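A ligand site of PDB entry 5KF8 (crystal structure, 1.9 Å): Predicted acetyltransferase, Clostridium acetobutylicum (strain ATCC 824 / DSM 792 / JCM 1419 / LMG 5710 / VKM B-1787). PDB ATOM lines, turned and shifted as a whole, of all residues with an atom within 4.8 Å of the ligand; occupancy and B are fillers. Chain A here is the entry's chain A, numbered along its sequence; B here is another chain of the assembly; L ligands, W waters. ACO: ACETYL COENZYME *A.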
ATOM      1  N   ILE A  20      23.270  10.849   6.202  1.00  0.00           N
ATOM      2  CA  ILE A  20      22.520  11.996   6.714  1.00  0.00           C
ATOM      3  C   ILE A  20      22.346  13.163   5.752  1.00  0.00           C
ATOM      4  O   ILE A  20      21.930  14.243   6.160  1.00  0.00           O
ATOM      5  CB  ILE A  20      23.110  12.486   8.067  1.00  0.00           C
ATOM      6  CG1 ILE A  20      24.444  13.250   7.842  1.00  0.00           C
ATOM      7  CG2 ILE A  20      23.244  11.307   9.035  1.00  0.00           C
ATOM      8  CD1 ILE A  20      25.107  13.705   9.144  1.00  0.00           C
ATOM      9  N   ILE A  78      34.369  15.976  19.864  1.00  0.00           N
ATOM     10  CA  ILE A  78      33.943  15.078  18.824  1.00  0.00           C
ATOM     11  C   ILE A  78      33.233  15.934  17.762  1.00  0.00           C
ATOM     12  O   ILE A  78      32.112  16.396  18.006  1.00  0.00           O
ATOM     13  CB  ILE A  78      33.006  14.008  19.353  1.00  0.00           C
ATOM     14  CG1 ILE A  78      33.578  13.321  20.610  1.00  0.00           C
ATOM     15  CG2 ILE A  78      32.702  12.997  18.255  1.00  0.00           C
ATOM     16  CD1 ILE A  78      34.907  12.654  20.402  1.00  0.00           C
ATOM     17  N   ASN A  79      33.924  16.193  16.664  1.00  0.00           N
ATOM     18  CA  ASN A  79      33.415  17.051  15.581  1.00  0.00           C
ATOM     19  C   ASN A  79      32.212  16.331  14.899  1.00  0.00           C
ATOM     20  O   ASN A  79      31.226  16.977  14.606  1.00  0.00           O
ATOM     21  CB  ASN A  79      34.511  17.339  14.586  1.00  0.00           C
ATOM     22  CG  ASN A  79      34.034  17.838  13.221  1.00  0.00           C
ATOM     23  OD1 ASN A  79      33.712  17.045  12.319  1.00  0.00           O
ATOM     24  ND2 ASN A  79      34.157  19.122  13.002  1.00  0.00           N
ATOM     25  N   SER A  80      32.373  15.060  14.579  1.00  0.00           N
ATOM     26  CA  SER A  80      31.345  14.256  14.026  1.00  0.00           C
ATOM     27  C   SER A  80      31.714  12.788  14.186  1.00  0.00           C
ATOM     28  O   SER A  80      32.900  12.427  14.289  1.00  0.00           O
ATOM     29  CB  SER A  80      31.193  14.578  12.535  1.00  0.00           C
ATOM     30  OG  SER A  80      32.453  14.585  11.887  1.00  0.00           O
ATOM     31  N   ILE A  81      30.683  11.966  14.135  1.00  0.00           N
ATOM     32  CA  ILE A  81      30.843  10.517  14.046  1.00  0.00           C
ATOM     33  C   ILE A  81      29.684   9.906  13.298  1.00  0.00           C
ATOM     34  O   ILE A  81      28.550  10.220  13.605  1.00  0.00           O
ATOM     35  CB  ILE A  81      30.998   9.873  15.450  1.00  0.00           C
ATOM     36  CG1 ILE A  81      31.099   8.325  15.346  1.00  0.00           C
ATOM     37  CG2 ILE A  81      29.875  10.212  16.415  1.00  0.00           C
ATOM     38  CD1 ILE A  81      31.548   7.701  16.665  1.00  0.00           C
ATOM     39  N   ILE A  82      29.948   9.088  12.278  1.00  0.00           N
ATOM     40  CA  ILE A  82      28.907   8.381  11.575  1.00  0.00           C
ATOM     41  C   ILE A  82      29.407   6.948  11.271  1.00  0.00           C
ATOM     42  O   ILE A  82      30.530   6.765  10.787  1.00  0.00           O
ATOM     43  CB  ILE A  82      28.529   9.058  10.235  1.00  0.00           C
ATOM     44  CG1 ILE A  82      28.346  10.590  10.394  1.00  0.00           C
ATOM     45  CG2 ILE A  82      27.311   8.376   9.668  1.00  0.00           C
ATOM     46  CD1 ILE A  82      28.046  11.344   9.086  1.00  0.00           C
ATOM     47  N   VAL A  83      28.531   5.977  11.553  1.00  0.00           N
ATOM     48  CA  VAL A  83      28.611   4.619  11.027  1.00  0.00           C
ATOM     49  C   VAL A  83      27.598   4.399   9.938  1.00  0.00           C
ATOM     50  O   VAL A  83      26.424   4.857  10.048  1.00  0.00           O
ATOM     51  CB  VAL A  83      28.415   3.648  12.196  1.00  0.00           C
ATOM     52  CG1 VAL A  83      28.283   2.203  11.721  1.00  0.00           C
ATOM     53  CG2 VAL A  83      29.605   3.814  13.136  1.00  0.00           C
ATOM     54  N   PHE A  87      25.795  -1.177   8.759  1.00  0.00           N
ATOM     55  CA  PHE A  87      26.751  -1.728   9.717  1.00  0.00           C
ATOM     56  C   PHE A  87      26.508  -1.267  11.129  1.00  0.00           C
ATOM     57  O   PHE A  87      27.402  -1.248  11.948  1.00  0.00           O
ATOM     58  CB  PHE A  87      28.164  -1.359   9.259  1.00  0.00           C
ATOM     59  CG  PHE A  87      28.513  -1.959   7.916  1.00  0.00           C
ATOM     60  CD1 PHE A  87      29.084  -3.237   7.835  1.00  0.00           C
ATOM     61  CD2 PHE A  87      28.267  -1.262   6.756  1.00  0.00           C
ATOM     62  CE1 PHE A  87      29.429  -3.808   6.596  1.00  0.00           C
ATOM     63  CE2 PHE A  87      28.571  -1.844   5.524  1.00  0.00           C
ATOM     64  CZ  PHE A  87      29.172  -3.102   5.446  1.00  0.00           C
ATOM     65  N   ARG A  88      25.274  -0.892  11.429  1.00  0.00           N
ATOM     66  CA  ARG A  88      24.925  -0.352  12.765  1.00  0.00           C
ATOM     67  C   ARG A  88      24.757  -1.464  13.768  1.00  0.00           C
ATOM     68  O   ARG A  88      24.501  -2.608  13.382  1.00  0.00           O
ATOM     69  CB  ARG A  88      23.567   0.403  12.740  1.00  0.00           C
ATOM     70  CG  ARG A  88      23.512   1.597  11.807  1.00  0.00           C
ATOM     71  CD  ARG A  88      24.117   2.822  12.459  1.00  0.00           C
ATOM     72  NE  ARG A  88      24.233   3.918  11.513  1.00  0.00           N
ATOM     73  CZ  ARG A  88      23.292   4.737  11.111  1.00  0.00           C
ATOM     74  NH1 ARG A  88      23.558   5.632  10.158  1.00  0.00           N
ATOM     75  NH2 ARG A  88      22.106   4.700  11.668  1.00  0.00           N
ATOM     76  N   HIS A  89      24.850  -1.108  15.043  1.00  0.00           N
ATOM     77  CA  HIS A  89      24.670  -2.025  16.097  1.00  0.00           C
ATOM     78  C   HIS A  89      25.583  -3.227  15.980  1.00  0.00           C
ATOM     79  O   HIS A  89      25.201  -4.322  16.391  1.00  0.00           O
ATOM     80  CB  HIS A  89      23.180  -2.430  16.265  1.00  0.00           C
ATOM     81  CG  HIS A  89      22.310  -1.310  16.748  1.00  0.00           C
ATOM     82  ND1 HIS A  89      22.211  -0.981  18.081  1.00  0.00           N
ATOM     83  CD2 HIS A  89      21.522  -0.440  16.077  1.00  0.00           C
ATOM     84  CE1 HIS A  89      21.387   0.039  18.212  1.00  0.00           C
ATOM     85  NE2 HIS A  89      20.962   0.397  17.014  1.00  0.00           N
ATOM     86  N   GLN A  90      26.824  -2.994  15.560  1.00  0.00           N
ATOM     87  CA  GLN A  90      27.881  -4.011  15.581  1.00  0.00           C
ATOM     88  C   GLN A  90      29.074  -3.597  16.469  1.00  0.00           C
ATOM     89  O   GLN A  90      30.091  -4.282  16.497  1.00  0.00           O
ATOM     90  CB  GLN A  90      28.404  -4.231  14.179  1.00  0.00           C
ATOM     91  CG  GLN A  90      27.366  -4.675  13.204  1.00  0.00           C
ATOM     92  CD  GLN A  90      27.974  -5.138  11.908  1.00  0.00           C
ATOM     93  OE1 GLN A  90      29.192  -5.257  11.749  1.00  0.00           O
ATOM     94  NE2 GLN A  90      27.117  -5.307  10.913  1.00  0.00           N
ATOM     95  N   GLY A  91      28.923  -2.494  17.204  1.00  0.00           N
ATOM     96  CA  GLY A  91      29.976  -1.998  18.075  1.00  0.00           C
ATOM     97  C   GLY A  91      30.972  -1.098  17.357  1.00  0.00           C
ATOM     98  O   GLY A  91      31.998  -0.718  17.932  1.00  0.00           O
ATOM     99  N   ILE A  92      30.719  -0.733  16.108  1.00  0.00           N
ATOM    100  CA  ILE A  92      31.736   0.009  15.373  1.00  0.00           C
ATOM    101  C   ILE A  92      31.824   1.444  15.936  1.00  0.00           C
ATOM    102  O   ILE A  92      32.937   1.936  16.144  1.00  0.00           O
ATOM    103  CB  ILE A  92      31.463   0.031  13.862  1.00  0.00           C
ATOM    104  CG1 ILE A  92      31.513  -1.439  13.342  1.00  0.00           C
ATOM    105  CG2 ILE A  92      32.418   0.999  13.171  1.00  0.00           C
ATOM    106  CD1 ILE A  92      30.966  -1.580  11.931  1.00  0.00           C
ATOM    107  N   GLY A  93      30.680   2.037  16.265  1.00  0.00           N
ATOM    108  CA  GLY A  93      30.667   3.369  16.851  1.00  0.00           C
ATOM    109  C   GLY A  93      31.418   3.410  18.170  1.00  0.00           C
ATOM    110  O   GLY A  93      32.220   4.338  18.434  1.00  0.00           O
ATOM    111  N   THR A  94      31.168   2.399  18.989  1.00  0.00           N
ATOM    112  CA  THR A  94      31.893   2.228  20.231  1.00  0.00           C
ATOM    113  C   THR A  94      33.433   2.163  20.042  1.00  0.00           C
ATOM    114  O   THR A  94      34.175   2.871  20.722  1.00  0.00           O
ATOM    115  CB  THR A  94      31.354   0.999  21.012  1.00  0.00           C
ATOM    116  OG1 THR A  94      29.943   1.143  21.217  1.00  0.00           O
ATOM    117  CG2 THR A  94      32.114   0.827  22.347  1.00  0.00           C
ATOM    118  N   CYS A 114      30.443  17.301  22.438  1.00  0.00           N
ATOM    119  CA  CYS A 114      29.837  16.919  21.197  1.00  0.00           C
ATOM    120  C   CYS A 114      29.667  18.179  20.388  1.00  0.00           C
ATOM    121  O   CYS A 114      28.852  19.030  20.761  1.00  0.00           O
ATOM    122  CB  CYS A 114      28.475  16.229  21.388  1.00  0.00           C
ATOM    123  SG  CYS A 114      28.669  14.577  22.103  1.00  0.00           S
ATOM    124  N   GLY A 115      30.369  18.221  19.255  1.00  0.00           N
ATOM    125  CA  GLY A 115      30.431  19.398  18.386  1.00  0.00           C
ATOM    126  C   GLY A 115      30.850  20.647  19.174  1.00  0.00           C
ATOM    127  O   GLY A 115      31.514  20.531  20.199  1.00  0.00           O
ATOM    128  N   PHE A 122      28.477  21.065  13.663  1.00  0.00           N
ATOM    129  CA  PHE A 122      27.289  21.058  14.485  1.00  0.00           C
ATOM    130  C   PHE A 122      27.572  21.824  15.795  1.00  0.00           C
ATOM    131  O   PHE A 122      28.602  21.608  16.462  1.00  0.00           O
ATOM    132  CB  PHE A 122      26.977  19.642  14.882  1.00  0.00           C
ATOM    133  CG  PHE A 122      26.855  18.677  13.737  1.00  0.00           C
ATOM    134  CD1 PHE A 122      25.889  18.848  12.756  1.00  0.00           C
ATOM    135  CD2 PHE A 122      27.634  17.544  13.712  1.00  0.00           C
ATOM    136  CE1 PHE A 122      25.733  17.929  11.726  1.00  0.00           C
ATOM    137  CE2 PHE A 122      27.458  16.604  12.689  1.00  0.00           C
ATOM    138  CZ  PHE A 122      26.542  16.807  11.694  1.00  0.00           C
ATOM    139  N   ILE A 125      24.603  17.990  19.470  1.00  0.00           N
ATOM    140  CA  ILE A 125      23.928  16.825  18.822  1.00  0.00           C
ATOM    141  C   ILE A 125      22.660  17.267  18.110  1.00  0.00           C
ATOM    142  O   ILE A 125      21.742  17.726  18.736  1.00  0.00           O
ATOM    143  CB  ILE A 125      23.570  15.723  19.817  1.00  0.00           C
ATOM    144  CG1 ILE A 125      24.814  15.324  20.603  1.00  0.00           C
ATOM    145  CG2 ILE A 125      22.877  14.544  19.116  1.00  0.00           C
ATOM    146  CD1 ILE A 125      24.479  14.344  21.765  1.00  0.00           C
ATOM    147  N   PRO A 126      22.610  17.188  16.778  1.00  0.00           N
ATOM    148  CA  PRO A 126      21.443  17.633  16.041  1.00  0.00           C
ATOM    149  C   PRO A 126      20.182  16.839  16.436  1.00  0.00           C
ATOM    150  O   PRO A 126      20.206  15.629  16.721  1.00  0.00           O
ATOM    151  CB  PRO A 126      21.819  17.341  14.563  1.00  0.00           C
ATOM    152  CG  PRO A 126      23.291  17.334  14.569  1.00  0.00           C
ATOM    153  CD  PRO A 126      23.561  16.594  15.846  1.00  0.00           C
ATOM    154  N   CYS A 129      19.650  13.783  14.730  1.00  0.00           N
ATOM    155  CA  CYS A 129      20.389  12.676  15.361  1.00  0.00           C
ATOM    156  C   CYS A 129      20.034  12.430  16.788  1.00  0.00           C
ATOM    157  O   CYS A 129      20.818  11.878  17.576  1.00  0.00           O
ATOM    158  CB  CYS A 129      21.886  12.982  15.263  1.00  0.00           C
ATOM    159  SG  CYS A 129      22.454  13.311  13.563  1.00  0.00           S
ATOM    160  N   PRO A 131      18.414  10.034  18.151  1.00  0.00           N
ATOM    161  CA  PRO A 131      18.635   8.702  18.713  1.00  0.00           C
ATOM    162  C   PRO A 131      20.105   8.461  19.175  1.00  0.00           C
ATOM    163  O   PRO A 131      20.335   7.597  20.033  1.00  0.00           O
ATOM    164  CB  PRO A 131      18.264   7.756  17.559  1.00  0.00           C
ATOM    165  CG  PRO A 131      17.230   8.548  16.787  1.00  0.00           C
ATOM    166  CD  PRO A 131      17.804   9.956  16.804  1.00  0.00           C
ATOM    167  N   SER A 132      21.064   9.173  18.605  1.00  0.00           N
ATOM    168  CA  SER A 132      22.424   9.073  19.069  1.00  0.00           C
ATOM    169  C   SER A 132      22.572   9.644  20.491  1.00  0.00           C
ATOM    170  O   SER A 132      23.552   9.339  21.146  1.00  0.00           O
ATOM    171  CB  SER A 132      23.380   9.797  18.128  1.00  0.00           C
ATOM    172  OG  SER A 132      23.326  11.208  18.288  1.00  0.00           O
ATOM    173  N   GLU A 134      21.238   8.621  23.134  1.00  0.00           N
ATOM    174  CA  GLU A 134      21.389   7.402  23.938  1.00  0.00           C
ATOM    175  C   GLU A 134      22.755   6.706  23.799  1.00  0.00           C
ATOM    176  O   GLU A 134      23.320   6.133  24.766  1.00  0.00           O
ATOM    177  CB  GLU A 134      20.294   6.430  23.524  1.00  0.00           C
ATOM    178  CG  GLU A 134      19.934   5.415  24.549  1.00  0.00           C
ATOM    179  CD  GLU A 134      19.566   6.046  25.885  1.00  0.00           C
ATOM    180  OE1 GLU A 134      18.694   6.982  25.953  1.00  0.00           O
ATOM    181  OE2 GLU A 134      20.202   5.554  26.845  1.00  0.00           O
ATOM    182  N   PHE A 135      23.251   6.698  22.571  1.00  0.00           N
ATOM    183  CA  PHE A 135      24.613   6.250  22.299  1.00  0.00           C
ATOM    184  C   PHE A 135      25.628   7.040  23.152  1.00  0.00           C
ATOM    185  O   PHE A 135      26.507   6.453  23.809  1.00  0.00           O
ATOM    186  CB  PHE A 135      24.921   6.352  20.803  1.00  0.00           C
ATOM    187  CG  PHE A 135      26.376   6.160  20.494  1.00  0.00           C
ATOM    188  CD1 PHE A 135      26.918   4.865  20.390  1.00  0.00           C
ATOM    189  CD2 PHE A 135      27.192   7.230  20.222  1.00  0.00           C
ATOM    190  CE1 PHE A 135      28.252   4.662  20.085  1.00  0.00           C
ATOM    191  CE2 PHE A 135      28.518   7.040  19.887  1.00  0.00           C
ATOM    192  CZ  PHE A 135      29.058   5.752  19.814  1.00  0.00           C
ATOM    193  N   PHE A 136      25.469   8.362  23.206  1.00  0.00           N
ATOM    194  CA  PHE A 136      26.387   9.201  23.979  1.00  0.00           C
ATOM    195  C   PHE A 136      26.158   9.056  25.494  1.00  0.00           C
ATOM    196  O   PHE A 136      27.114   8.900  26.255  1.00  0.00           O
ATOM    197  CB  PHE A 136      26.343  10.675  23.502  1.00  0.00           C
ATOM    198  CG  PHE A 136      26.926  10.916  22.126  1.00  0.00           C
ATOM    199  CD1 PHE A 136      28.307  10.903  21.915  1.00  0.00           C
ATOM    200  CD2 PHE A 136      26.085  11.180  21.040  1.00  0.00           C
ATOM    201  CE1 PHE A 136      28.845  11.100  20.652  1.00  0.00           C
ATOM    202  CE2 PHE A 136      26.623  11.368  19.766  1.00  0.00           C
ATOM    203  CZ  PHE A 136      27.973  11.353  19.574  1.00  0.00           C
ATOM    204  N   VAL A 138      25.066   6.360  27.119  1.00  0.00           N
ATOM    205  CA  VAL A 138      25.717   5.091  27.485  1.00  0.00           C
ATOM    206  C   VAL A 138      27.208   5.287  27.737  1.00  0.00           C
ATOM    207  O   VAL A 138      27.759   4.580  28.557  1.00  0.00           O
ATOM    208  CB  VAL A 138      25.503   4.007  26.404  1.00  0.00           C
ATOM    209  CG1 VAL A 138      26.496   2.870  26.509  1.00  0.00           C
ATOM    210  CG2 VAL A 138      24.067   3.503  26.472  1.00  0.00           C
ATOM    211  N   ASN B 295      13.432   4.475  16.407  1.00  0.00           N
ATOM    212  CA  ASN B 295      14.449   3.508  15.999  1.00  0.00           C
ATOM    213  C   ASN B 295      13.928   2.436  15.065  1.00  0.00           C
ATOM    214  O   ASN B 295      14.672   1.883  14.290  1.00  0.00           O
ATOM    215  CB  ASN B 295      15.072   2.823  17.238  1.00  0.00           C
ATOM    216  CG  ASN B 295      16.113   3.690  17.949  1.00  0.00           C
ATOM    217  OD1 ASN B 295      16.439   3.492  19.151  1.00  0.00           O
ATOM    218  ND2 ASN B 295      16.669   4.630  17.227  1.00  0.00           N
HETATM  219  N1A ACO L   1      19.223   4.260  20.061  1.00  0.00           N
HETATM  220  C2A ACO L   1      19.506   3.936  21.306  1.00  0.00           C
HETATM  221  N3A ACO L   1      20.698   3.500  21.703  1.00  0.00           N
HETATM  222  C4A ACO L   1      21.689   3.373  20.817  1.00  0.00           C
HETATM  223  C5A ACO L   1      21.453   3.735  19.417  1.00  0.00           C
HETATM  224  C6A ACO L   1      20.089   4.167  19.052  1.00  0.00           C
HETATM  225  N6A ACO L   1      19.827   4.503  17.789  1.00  0.00           N
HETATM  226  N7A ACO L   1      22.582   3.520  18.778  1.00  0.00           N
HETATM  227  C8A ACO L   1      23.462   3.079  19.654  1.00  0.00           C
HETATM  228  N9A ACO L   1      22.957   3.017  20.873  1.00  0.00           N
HETATM  229  C1B ACO L   1      23.630   2.535  22.108  1.00  0.00           C
HETATM  230  C2B ACO L   1      23.154   1.095  22.364  1.00  0.00           C
HETATM  231  O2B ACO L   1      23.263   0.779  23.713  1.00  0.00           O
HETATM  232  C3B ACO L   1      24.184   0.260  21.679  1.00  0.00           C
HETATM  233  O3B ACO L   1      24.252  -1.075  22.083  1.00  0.00           O
HETATM  234  P3B ACO L   1      23.285  -2.166  21.490  1.00  0.00           P
HETATM  235  O7A ACO L   1      23.525  -2.504  20.142  1.00  0.00           O
HETATM  236  O8A ACO L   1      23.510  -3.271  22.431  1.00  0.00           O
HETATM  237  O9A ACO L   1      21.960  -1.710  21.603  1.00  0.00           O
HETATM  238  C4B ACO L   1      25.424   1.094  21.983  1.00  0.00           C
HETATM  239  O4B ACO L   1      25.007   2.430  21.997  1.00  0.00           O
HETATM  240  C5B ACO L   1      26.538   0.786  21.011  1.00  0.00           C
HETATM  241  O5B ACO L   1      26.197   1.016  19.702  1.00  0.00           O
HETATM  242  P1A ACO L   1      27.210   0.829  18.557  1.00  0.00           P
HETATM  243  O1A ACO L   1      26.847  -0.340  17.862  1.00  0.00           O
HETATM  244  O2A ACO L   1      28.492   0.954  18.983  1.00  0.00           O
HETATM  245  O3A ACO L   1      26.865   2.053  17.625  1.00  0.00           O
HETATM  246  P2A ACO L   1      26.874   2.209  16.091  1.00  0.00           P
HETATM  247  O4A ACO L   1      27.989   1.591  15.537  1.00  0.00           O
HETATM  248  O5A ACO L   1      25.681   1.722  15.659  1.00  0.00           O
HETATM  249  O6A ACO L   1      26.917   3.760  15.909  1.00  0.00           O
HETATM  250  CBP ACO L   1      25.999   5.971  15.750  1.00  0.00           C
HETATM  251  CCP ACO L   1      26.186   4.713  16.621  1.00  0.00           C
HETATM  252  CDP ACO L   1      27.379   6.440  15.373  1.00  0.00           C
HETATM  253  CEP ACO L   1      25.294   7.013  16.563  1.00  0.00           C
HETATM  254  CAP ACO L   1      25.225   5.624  14.465  1.00  0.00           C
HETATM  255  OAP ACO L   1      23.935   5.313  14.865  1.00  0.00           O
HETATM  256  C9P ACO L   1      25.165   6.739  13.432  1.00  0.00           C
HETATM  257  O9P ACO L   1      26.031   6.891  12.653  1.00  0.00           O
HETATM  258  N8P ACO L   1      24.064   7.436  13.473  1.00  0.00           N
HETATM  259  C7P ACO L   1      23.775   8.550  12.621  1.00  0.00           C
HETATM  260  C6P ACO L   1      24.775   9.661  12.704  1.00  0.00           C
HETATM  261  C5P ACO L   1      24.705  10.308  14.075  1.00  0.00           C
HETATM  262  O5P ACO L   1      23.709  10.472  14.633  1.00  0.00           O
HETATM  263  N4P ACO L   1      25.864  10.644  14.590  1.00  0.00           N
HETATM  264  C3P ACO L   1      26.085  11.489  15.735  1.00  0.00           C
HETATM  265  C2P ACO L   1      25.839  12.983  15.513  1.00  0.00           C
HETATM  266  S1P ACO L   1      26.326  14.139  16.767  1.00  0.00           S
HETATM  267  C   ACO L   1      27.995  14.261  16.615  1.00  0.00           C
HETATM  268  O   ACO L   1      28.562  13.695  15.770  1.00  0.00           O
HETATM  269  CH3 ACO L   1      28.777  15.154  17.529  1.00  0.00           C
HETATM  270  O   HOH W   1      26.164  -2.545  19.330  1.00  0.00           O
HETATM  271  O   HOH W   2      17.659   6.547  21.140  1.00  0.00           O
HETATM  272  O   HOH W   3      21.185   9.292  15.037  1.00  0.00           O
HETATM  273  O   HOH W   4      18.746   1.583  16.718  1.00  0.00           O
HETATM  274  O   HOH W   5      23.398  -4.895  19.054  1.00  0.00           O
HETATM  275  O   HOH W   6      21.386   6.718  15.546  1.00  0.00           O
HETATM  276  O   HOH W   7      24.171  -1.901  24.714  1.00  0.00           O
HETATM  277  O   HOH W   8      23.176   2.944  16.008  1.00  0.00           O
HETATM  278  O   HOH W   9      25.364  -5.148  21.815  1.00  0.00           O
HETATM  279  O   HOH W  10      28.230  -0.884  14.486  1.00  0.00           O
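The guanidinium group (NE) of Arg 88 sits at hydrogen-bond distance from the backbone carbonyl oxygen (O) of Val 83. OG of Ser 132 is in hydrogen-bond range of O of Cys 129. The side-chain amide oxygen of Asn 79 is in hydrogen-bond range of the side-chain hydroxyl of Ser 80 (2.8 Å). The backbone carbonyl oxygen (O) of Ile 78 lies within hydrogen-bond range of the backbone NH (N) of Gly 115 (2.8 Å).
Water W5 bridges an oxygen (O7A) of the ligand and the backbone carbonyl oxygen of His 89. Water W1 lies within hydrogen-bond range of O1A of the ligand (2.7 Å) and N of Gly 91 (3.5 Å). Water W2 bridges N1A of the ligand (3.0 Å) and O of Pro 131 (3.1 Å). Water W4 lies within hydrogen-bond range of NE2 of His 89 (2.5 Å) and N6A of the ligand (3.3 Å).
Merely in contact with the ligand: Ser 80, Ile 82, Glu 134, Arg 88, Phe 135, Gln 90, Pro 131, Ser 132, Ile 78, Ile 92, Pro 126, Gly 115 and Val 138. Hydrophobic or aromatic side chains within 4 Å of the ligand: Ile 81, Ile 82, Val 83, His 89, Pro 126, Pro 131, Phe 135 and Val 138. Within 4 Å of the ligand: Ile 78, Ser 80, Ile 81, Ile 82, Val 83, Arg 88, His 89, Gln 90, Gly 91, Ile 92, Gly 93, Thr 94, Gly 115, Pro 126, Cys 129, Pro 131, Ser 132, Glu 134, Phe 135, Val 138 and Asn 295 of chain B. Along chain A the residues within 4 Å of the ligand span positions 78 to 138.
N of Thr 94 sits at hydrogen-bond distance from O2A of the ligand (3.0 Å). The side-chain hydroxyl (OG1) of Thr 94 is in hydrogen-bond range of an oxygen (O2A) of the ligand, 2.7 Å away. O4A of the ligand sits at hydrogen-bond distance from N of Gly 93, 2.8 Å away. The backbone NH of His 89 is in hydrogen-bond range of an oxygen (O5A) of the ligand (3.0 Å). An oxygen (O7A) of the ligand is in hydrogen-bond range of a ring nitrogen (ND1) of His 89 (2.9 Å). An oxygen (O9P) of the ligand is in hydrogen-bond range of the backbone NH of Val 83, 2.9 Å away. The backbone NH (N) of Ile 81 sits at hydrogen-bond distance from an oxygen (O) of the ligand (3.2 Å). O of Ile 81 sits at hydrogen-bond distance from N4P of the ligand (2.9 Å). The side-chain amide oxygen (OD1) of Asn 295 of chain B sits close to a nitrogen (N1A) of the ligand (3.0 Å). An oxygen (O1A) of the ligand sits at hydrogen-bond distance from the backbone NH (N) of Gly 91 (3.1 Å). The side-chain sulfur (SG) of Cys 129 lies close to an oxygen (O5P) of the ligand, 3.3 Å away.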
